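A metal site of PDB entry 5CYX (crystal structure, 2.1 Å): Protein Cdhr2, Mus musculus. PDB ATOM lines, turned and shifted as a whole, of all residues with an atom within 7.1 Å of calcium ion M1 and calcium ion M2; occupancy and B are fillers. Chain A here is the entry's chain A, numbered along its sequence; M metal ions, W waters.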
ATOM      1  N   GLU A 116     -30.474   1.660 -14.435  1.00  0.00           N
ATOM      2  CA  GLU A 116     -30.733   0.217 -14.302  1.00  0.00           C
ATOM      3  C   GLU A 116     -32.030  -0.031 -13.504  1.00  0.00           C
ATOM      4  O   GLU A 116     -32.613  -1.083 -13.699  1.00  0.00           O
ATOM      5  CB  GLU A 116     -29.577  -0.549 -13.686  1.00  0.00           C
ATOM      6  CG  GLU A 116     -29.387  -0.431 -12.183  1.00  0.00           C
ATOM      7  CD  GLU A 116     -28.101  -1.079 -11.647  1.00  0.00           C
ATOM      8  OE1 GLU A 116     -27.585  -2.144 -12.153  1.00  0.00           O
ATOM      9  OE2 GLU A 116     -27.631  -0.531 -10.616  1.00  0.00           O
ATOM     10  N   SER A 173     -29.560  -4.949 -15.043  1.00  0.00           N
ATOM     11  CA  SER A 173     -28.485  -4.899 -14.028  1.00  0.00           C
ATOM     12  C   SER A 173     -27.138  -4.601 -14.672  1.00  0.00           C
ATOM     13  O   SER A 173     -26.610  -5.447 -15.404  1.00  0.00           O
ATOM     14  CB  SER A 173     -28.363  -6.221 -13.245  1.00  0.00           C
ATOM     15  OG  SER A 173     -27.300  -6.101 -12.277  1.00  0.00           O
ATOM     16  N   TYR A 174     -26.602  -3.410 -14.403  1.00  0.00           N
ATOM     17  CA  TYR A 174     -25.276  -3.033 -14.867  1.00  0.00           C
ATOM     18  C   TYR A 174     -24.220  -4.092 -14.519  1.00  0.00           C
ATOM     19  O   TYR A 174     -23.425  -4.440 -15.341  1.00  0.00           O
ATOM     20  CB  TYR A 174     -24.864  -1.641 -14.310  1.00  0.00           C
ATOM     21  CG  TYR A 174     -23.442  -1.205 -14.649  1.00  0.00           C
ATOM     22  CD1 TYR A 174     -22.345  -1.697 -13.963  1.00  0.00           C
ATOM     23  CD2 TYR A 174     -23.188  -0.250 -15.646  1.00  0.00           C
ATOM     24  CE1 TYR A 174     -21.030  -1.277 -14.283  1.00  0.00           C
ATOM     25  CE2 TYR A 174     -21.887   0.142 -15.983  1.00  0.00           C
ATOM     26  CZ  TYR A 174     -20.819  -0.353 -15.286  1.00  0.00           C
ATOM     27  OH  TYR A 174     -19.512   0.059 -15.592  1.00  0.00           O
ATOM     28  N   ASN A 175     -24.207  -4.559 -13.292  1.00  0.00           N
ATOM     29  CA  ASN A 175     -23.215  -5.499 -12.757  1.00  0.00           C
ATOM     30  C   ASN A 175     -23.503  -7.000 -12.977  1.00  0.00           C
ATOM     31  O   ASN A 175     -22.591  -7.778 -13.072  1.00  0.00           O
ATOM     32  CB  ASN A 175     -23.102  -5.250 -11.254  1.00  0.00           C
ATOM     33  CG  ASN A 175     -22.568  -3.873 -10.969  1.00  0.00           C
ATOM     34  OD1 ASN A 175     -23.321  -2.902 -10.674  1.00  0.00           O
ATOM     35  ND2 ASN A 175     -21.295  -3.743 -11.151  1.00  0.00           N
ATOM     36  N   ILE A 213     -26.909   2.636 -16.796  1.00  0.00           N
ATOM     37  CA  ILE A 213     -26.265   3.422 -15.752  1.00  0.00           C
ATOM     38  C   ILE A 213     -26.364   2.679 -14.435  1.00  0.00           C
ATOM     39  O   ILE A 213     -27.459   2.248 -13.995  1.00  0.00           O
ATOM     40  CB  ILE A 213     -26.955   4.791 -15.612  1.00  0.00           C
ATOM     41  CG1 ILE A 213     -26.730   5.633 -16.868  1.00  0.00           C
ATOM     42  CG2 ILE A 213     -26.530   5.548 -14.346  1.00  0.00           C
ATOM     43  CD1 ILE A 213     -27.647   6.854 -16.934  1.00  0.00           C
ATOM     44  N   ASP A 214     -25.219   2.502 -13.803  1.00  0.00           N
ATOM     45  CA  ASP A 214     -25.130   1.783 -12.557  1.00  0.00           C
ATOM     46  C   ASP A 214     -25.647   2.704 -11.444  1.00  0.00           C
ATOM     47  O   ASP A 214     -25.240   3.892 -11.339  1.00  0.00           O
ATOM     48  CB  ASP A 214     -23.701   1.344 -12.274  1.00  0.00           C
ATOM     49  CG  ASP A 214     -23.604   0.251 -11.220  1.00  0.00           C
ATOM     50  OD1 ASP A 214     -24.683  -0.239 -10.670  1.00  0.00           O
ATOM     51  OD2 ASP A 214     -22.452  -0.117 -10.959  1.00  0.00           O
ATOM     52  N   GLU A 215     -26.568   2.154 -10.645  1.00  0.00           N
ATOM     53  CA  GLU A 215     -27.123   2.890  -9.510  1.00  0.00           C
ATOM     54  C   GLU A 215     -26.751   2.193  -8.199  1.00  0.00           C
ATOM     55  O   GLU A 215     -26.482   1.021  -8.218  1.00  0.00           O
ATOM     56  CB  GLU A 215     -28.627   3.007  -9.632  1.00  0.00           C
ATOM     57  CG  GLU A 215     -29.091   3.911 -10.774  1.00  0.00           C
ATOM     58  CD  GLU A 215     -30.616   3.978 -10.804  1.00  0.00           C
ATOM     59  OE1 GLU A 215     -31.298   3.071 -11.323  1.00  0.00           O
ATOM     60  OE2 GLU A 215     -31.149   4.947 -10.250  1.00  0.00           O
ATOM     61  N   PRO A 216     -26.664   2.945  -7.094  1.00  0.00           N
ATOM     62  CA  PRO A 216     -26.120   2.346  -5.889  1.00  0.00           C
ATOM     63  C   PRO A 216     -27.159   1.480  -5.159  1.00  0.00           C
ATOM     64  O   PRO A 216     -27.949   1.999  -4.378  1.00  0.00           O
ATOM     65  CB  PRO A 216     -25.699   3.539  -5.063  1.00  0.00           C
ATOM     66  CG  PRO A 216     -26.572   4.662  -5.522  1.00  0.00           C
ATOM     67  CD  PRO A 216     -26.853   4.404  -6.971  1.00  0.00           C
ATOM     68  N   ASP A 217     -27.169   0.187  -5.481  1.00  0.00           N
ATOM     69  CA  ASP A 217     -28.095  -0.753  -4.838  1.00  0.00           C
ATOM     70  C   ASP A 217     -27.502  -2.110  -4.523  1.00  0.00           C
ATOM     71  O   ASP A 217     -28.246  -3.048  -4.324  1.00  0.00           O
ATOM     72  CB  ASP A 217     -29.319  -0.946  -5.746  1.00  0.00           C
ATOM     73  CG  ASP A 217     -28.975  -1.576  -7.099  1.00  0.00           C
ATOM     74  OD1 ASP A 217     -27.781  -1.730  -7.502  1.00  0.00           O
ATOM     75  OD2 ASP A 217     -29.938  -1.916  -7.777  1.00  0.00           O
ATOM     76  N   LEU A 218     -26.181  -2.202  -4.492  1.00  0.00           N
ATOM     77  CA  LEU A 218     -25.507  -3.406  -4.066  1.00  0.00           C
ATOM     78  C   LEU A 218     -24.595  -3.014  -2.928  1.00  0.00           C
ATOM     79  O   LEU A 218     -23.880  -1.968  -2.986  1.00  0.00           O
ATOM     80  CB  LEU A 218     -24.732  -3.999  -5.239  1.00  0.00           C
ATOM     81  CG  LEU A 218     -25.573  -4.522  -6.396  1.00  0.00           C
ATOM     82  CD1 LEU A 218     -24.671  -4.886  -7.559  1.00  0.00           C
ATOM     83  CD2 LEU A 218     -26.365  -5.751  -5.959  1.00  0.00           C
ATOM     84  N   ASP A 219     -24.600  -3.838  -1.884  1.00  0.00           N
ATOM     85  CA  ASP A 219     -23.785  -3.576  -0.712  1.00  0.00           C
ATOM     86  C   ASP A 219     -22.302  -3.830  -1.012  1.00  0.00           C
ATOM     87  O   ASP A 219     -21.975  -4.512  -1.974  1.00  0.00           O
ATOM     88  CB  ASP A 219     -24.256  -4.437   0.488  1.00  0.00           C
ATOM     89  CG  ASP A 219     -25.587  -3.940   1.110  1.00  0.00           C
ATOM     90  OD1 ASP A 219     -26.005  -2.782   0.865  1.00  0.00           O
ATOM     91  OD2 ASP A 219     -26.195  -4.717   1.871  1.00  0.00           O
ATOM     92  N   PRO A 220     -21.392  -3.263  -0.191  1.00  0.00           N
ATOM     93  CA  PRO A 220     -19.955  -3.565  -0.294  1.00  0.00           C
ATOM     94  C   PRO A 220     -19.585  -4.965   0.158  1.00  0.00           C
ATOM     95  O   PRO A 220     -20.269  -5.525   1.006  1.00  0.00           O
ATOM     96  CB  PRO A 220     -19.334  -2.554   0.657  1.00  0.00           C
ATOM     97  CG  PRO A 220     -20.383  -2.340   1.680  1.00  0.00           C
ATOM     98  CD  PRO A 220     -21.676  -2.333   0.920  1.00  0.00           C
ATOM     99  N   VAL A 247     -15.016  -3.443  -0.755  1.00  0.00           N
ATOM    100  CA  VAL A 247     -15.212  -2.582  -1.915  1.00  0.00           C
ATOM    101  C   VAL A 247     -16.661  -2.611  -2.371  1.00  0.00           C
ATOM    102  O   VAL A 247     -17.370  -3.609  -2.186  1.00  0.00           O
ATOM    103  CB  VAL A 247     -14.289  -2.952  -3.107  1.00  0.00           C
ATOM    104  CG1 VAL A 247     -12.816  -2.868  -2.681  1.00  0.00           C
ATOM    105  CG2 VAL A 247     -14.588  -4.337  -3.632  1.00  0.00           C
ATOM    106  N   ASP A 248     -17.067  -1.523  -2.997  1.00  0.00           N
ATOM    107  CA  ASP A 248     -18.414  -1.342  -3.498  1.00  0.00           C
ATOM    108  C   ASP A 248     -18.675  -2.335  -4.639  1.00  0.00           C
ATOM    109  O   ASP A 248     -17.910  -2.387  -5.594  1.00  0.00           O
ATOM    110  CB  ASP A 248     -18.562   0.099  -3.969  1.00  0.00           C
ATOM    111  CG  ASP A 248     -19.913   0.423  -4.488  1.00  0.00           C
ATOM    112  OD1 ASP A 248     -20.825  -0.408  -4.340  1.00  0.00           O
ATOM    113  OD2 ASP A 248     -20.068   1.543  -5.027  1.00  0.00           O
ATOM    114  N   SER A 249     -19.759  -3.118  -4.510  1.00  0.00           N
ATOM    115  CA  SER A 249     -20.127  -4.069  -5.556  1.00  0.00           C
ATOM    116  C   SER A 249     -20.693  -3.395  -6.783  1.00  0.00           C
ATOM    117  O   SER A 249     -20.738  -4.000  -7.847  1.00  0.00           O
ATOM    118  CB  SER A 249     -21.109  -5.126  -5.012  1.00  0.00           C
ATOM    119  OG  SER A 249     -20.526  -5.772  -3.930  1.00  0.00           O
ATOM    120  N   ASP A 250     -21.107  -2.122  -6.664  1.00  0.00           N
ATOM    121  CA  ASP A 250     -21.539  -1.371  -7.822  1.00  0.00           C
ATOM    122  C   ASP A 250     -20.271  -0.853  -8.528  1.00  0.00           C
ATOM    123  O   ASP A 250     -19.717   0.235  -8.203  1.00  0.00           O
ATOM    124  CB  ASP A 250     -22.502  -0.223  -7.444  1.00  0.00           C
ATOM    125  CG  ASP A 250     -23.723  -0.694  -6.647  1.00  0.00           C
ATOM    126  OD1 ASP A 250     -24.616  -1.249  -7.229  1.00  0.00           O
ATOM    127  OD2 ASP A 250     -23.771  -0.509  -5.405  1.00  0.00           O
ATOM    128  N   LYS A 251     -19.847  -1.601  -9.539  1.00  0.00           N
ATOM    129  CA  LYS A 251     -18.554  -1.375 -10.218  1.00  0.00           C
ATOM    130  C   LYS A 251     -18.591  -0.165 -11.164  1.00  0.00           C
ATOM    131  O   LYS A 251     -17.564   0.284 -11.566  1.00  0.00           O
ATOM    132  CB  LYS A 251     -18.059  -2.617 -10.977  1.00  0.00           C
ATOM    133  CG  LYS A 251     -17.976  -3.886 -10.157  1.00  0.00           C
ATOM    134  CD  LYS A 251     -16.956  -3.808  -9.045  1.00  0.00           C
ATOM    135  CE  LYS A 251     -16.947  -5.114  -8.250  1.00  0.00           C
ATOM    136  NZ  LYS A 251     -16.271  -4.955  -6.942  1.00  0.00           N
ATOM    137  N   GLY A 252     -19.766   0.304 -11.522  1.00  0.00           N
ATOM    138  CA  GLY A 252     -19.911   1.554 -12.233  1.00  0.00           C
ATOM    139  C   GLY A 252     -19.841   2.789 -11.347  1.00  0.00           C
ATOM    140  O   GLY A 252     -19.875   3.894 -11.846  1.00  0.00           O
ATOM    141  N   ILE A 253     -19.757   2.578 -10.046  1.00  0.00           N
ATOM    142  CA  ILE A 253     -19.775   3.594  -9.044  1.00  0.00           C
ATOM    143  C   ILE A 253     -18.483   3.579  -8.252  1.00  0.00           C
ATOM    144  O   ILE A 253     -17.841   4.610  -8.175  1.00  0.00           O
ATOM    145  CB  ILE A 253     -21.052   3.513  -8.133  1.00  0.00           C
ATOM    146  CG1 ILE A 253     -22.297   3.854  -8.959  1.00  0.00           C
ATOM    147  CG2 ILE A 253     -21.003   4.533  -6.987  1.00  0.00           C
ATOM    148  CD1 ILE A 253     -23.643   3.408  -8.360  1.00  0.00           C
ATOM    149  N   ASN A 254     -18.092   2.448  -7.695  1.00  0.00           N
ATOM    150  CA  ASN A 254     -16.926   2.347  -6.771  1.00  0.00           C
ATOM    151  C   ASN A 254     -16.863   3.519  -5.776  1.00  0.00           C
ATOM    152  O   ASN A 254     -15.901   4.298  -5.762  1.00  0.00           O
ATOM    153  CB  ASN A 254     -15.558   2.225  -7.486  1.00  0.00           C
ATOM    154  CG  ASN A 254     -15.637   1.529  -8.807  1.00  0.00           C
ATOM    155  OD1 ASN A 254     -15.829   0.295  -8.866  1.00  0.00           O
ATOM    156  ND2 ASN A 254     -15.436   2.285  -9.895  1.00  0.00           N
ATOM    157  N   ASP A 255     -17.907   3.594  -4.961  1.00  0.00           N
ATOM    158  CA  ASP A 255     -18.095   4.551  -3.875  1.00  0.00           C
ATOM    159  C   ASP A 255     -17.015   4.251  -2.847  1.00  0.00           C
ATOM    160  O   ASP A 255     -16.671   3.086  -2.648  1.00  0.00           O
ATOM    161  CB  ASP A 255     -19.490   4.325  -3.232  1.00  0.00           C
ATOM    162  CG  ASP A 255     -19.958   5.496  -2.357  1.00  0.00           C
ATOM    163  OD1 ASP A 255     -19.241   6.496  -2.181  1.00  0.00           O
ATOM    164  OD2 ASP A 255     -21.084   5.397  -1.814  1.00  0.00           O
ATOM    165  N   GLU A 304     -20.556   2.250   2.908  1.00  0.00           N
ATOM    166  CA  GLU A 304     -20.340   3.145   1.796  1.00  0.00           C
ATOM    167  C   GLU A 304     -20.599   4.560   2.254  1.00  0.00           C
ATOM    168  O   GLU A 304     -21.345   4.791   3.195  1.00  0.00           O
ATOM    169  CB  GLU A 304     -21.203   2.779   0.597  1.00  0.00           C
ATOM    170  CG  GLU A 304     -20.771   1.448  -0.011  1.00  0.00           C
ATOM    171  CD  GLU A 304     -21.637   0.942  -1.158  1.00  0.00           C
ATOM    172  OE1 GLU A 304     -22.381   1.718  -1.769  1.00  0.00           O
ATOM    173  OE2 GLU A 304     -21.511  -0.230  -1.519  1.00  0.00           O
ATOM    174  N   ASN A 306     -21.962   7.130   0.545  1.00  0.00           N
ATOM    175  CA  ASN A 306     -23.253   7.600   0.114  1.00  0.00           C
ATOM    176  C   ASN A 306     -24.337   6.569   0.376  1.00  0.00           C
ATOM    177  O   ASN A 306     -24.079   5.352   0.414  1.00  0.00           O
ATOM    178  CB  ASN A 306     -23.210   7.944  -1.372  1.00  0.00           C
ATOM    179  CG  ASN A 306     -22.203   9.053  -1.658  1.00  0.00           C
ATOM    180  OD1 ASN A 306     -21.047   8.798  -2.005  1.00  0.00           O
ATOM    181  ND2 ASN A 306     -22.615  10.273  -1.412  1.00  0.00           N
ATOM    182  N   ASN A 308     -27.721   4.392  -0.351  1.00  0.00           N
ATOM    183  CA  ASN A 308     -28.205   3.675  -1.508  1.00  0.00           C
ATOM    184  C   ASN A 308     -29.459   4.343  -2.088  1.00  0.00           C
ATOM    185  O   ASN A 308     -29.925   5.337  -1.549  1.00  0.00           O
ATOM    186  CB  ASN A 308     -28.363   2.170  -1.189  1.00  0.00           C
ATOM    187  CG  ASN A 308     -29.513   1.838  -0.214  1.00  0.00           C
ATOM    188  OD1 ASN A 308     -30.445   2.621   0.028  1.00  0.00           O
ATOM    189  ND2 ASN A 308     -29.455   0.648   0.318  1.00  0.00           N
ATOM    190  N   ILE A 309     -29.963   3.809  -3.191  1.00  0.00           N
ATOM    191  CA  ILE A 309     -31.171   4.338  -3.845  1.00  0.00           C
ATOM    192  C   ILE A 309     -32.411   4.422  -2.945  1.00  0.00           C
ATOM    193  O   ILE A 309     -33.293   5.221  -3.214  1.00  0.00           O
ATOM    194  CB  ILE A 309     -31.566   3.532  -5.113  1.00  0.00           C
ATOM    195  CG1 ILE A 309     -31.833   2.051  -4.806  1.00  0.00           C
ATOM    196  CG2 ILE A 309     -30.501   3.662  -6.178  1.00  0.00           C
ATOM    197  CD1 ILE A 309     -32.435   1.329  -5.983  1.00  0.00           C
ATOM    198  N   ALA A 314     -25.442   1.340   2.970  1.00  0.00           N
ATOM    199  CA  ALA A 314     -24.972   0.160   2.275  1.00  0.00           C
ATOM    200  C   ALA A 314     -23.778  -0.295   3.075  1.00  0.00           C
ATOM    201  O   ALA A 314     -22.741   0.385   3.091  1.00  0.00           O
ATOM    202  CB  ALA A 314     -24.584   0.511   0.851  1.00  0.00           C
HETATM  203 CA    CA M   1     -26.102  -1.082  -9.025  1.00  0.00          CA
HETATM  204 CA    CA M   2     -23.010   0.127  -3.446  1.00  0.00          CA
HETATM  205  O   HOH W   1     -26.082  -3.119 -10.240  1.00  0.00           O
HETATM  206  O   HOH W   2     -22.615   2.269  -4.655  1.00  0.00           O
HETATM  207  O   HOH W   3     -25.280   0.875  -2.568  1.00  0.00           O
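N of Glu 116 lies within hydrogen-bond range of O of Ile 213, at 3.1 Å. The backbone NH (N) of Glu 304 lies within hydrogen-bond range of the backbone carbonyl oxygen (O) of Ala 314 (2.9 Å). The side-chain carboxylate (OD2) of Asp 248 lies within hydrogen-bond range of the backbone NH (N) of Asn 254 (3.4 Å). The side-chain carboxylate (OD2) of Asp 214 sits at hydrogen-bond distance from the backbone NH (N) of Gly 252 (2.8 Å). The backbone NH (N) of Lys 251 lies close to the side-chain amide nitrogen (ND2) of Asn 175 (3.0 Å). The backbone NH of Lys 251 lies within hydrogen-bond range of the side-chain carboxylate of Asp 214, 3.3 Å away. The side-chain amide oxygen (OD1) of Asn 175 lies close to the side-chain carboxylate (OD2) of Asp 214, 2.9 Å away. The side-chain carboxylate (OE1) of Glu 116 is in hydrogen-bond range of the backbone NH (N) of Tyr 174.
Residues that only touch calcium ion M1: Asn 175 (3.7 Å). Of the 26 residues printed, 6 come within 4 Å of calcium ion M1. The nearest printed residue that does not touch calcium ion M1 is Leu 218 (4.3 Å).
Four residues have an atom within 4 Å of calcium ion M2: Leu 218, Asp 248, Asp 250 and Glu 304.
Calcium ion M1 is bound by the side-chain carboxylate (OE2) of Glu 116 (2.3 Å), the backbone carbonyl oxygen (O) of Glu 215 (2.3 Å), the side-chain carboxylate (OD1) of Asp 214 (2.3 Å), the side-chain carboxylate (OD1) of Asp 250 (2.3 Å), the side-chain carboxylate (OD1) of Asp 217 (2.4 Å) and water W1 (2.4 Å).
Calcium ion M2 is bound by the side-chain carboxylate (OD2) of Asp 250 (2.2 Å). Calcium ion M2 is bound by O of Leu 218, at 2.3 Å. OE1 of Glu 304 is bound to calcium ion M2 (2.4 Å). OD1 of Asp 248 binds calcium ion M2, 2.4 Å away. Calcium ion M2 is bound by OE2 of Glu 304 (2.5 Å). Water W2 is bound to calcium ion M2 (2.5 Å). Water W3 is bound to calcium ion M2, at 2.5 Å.
Water W1 bridges OE1 of Glu 116 and OD1 of Asn 175.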
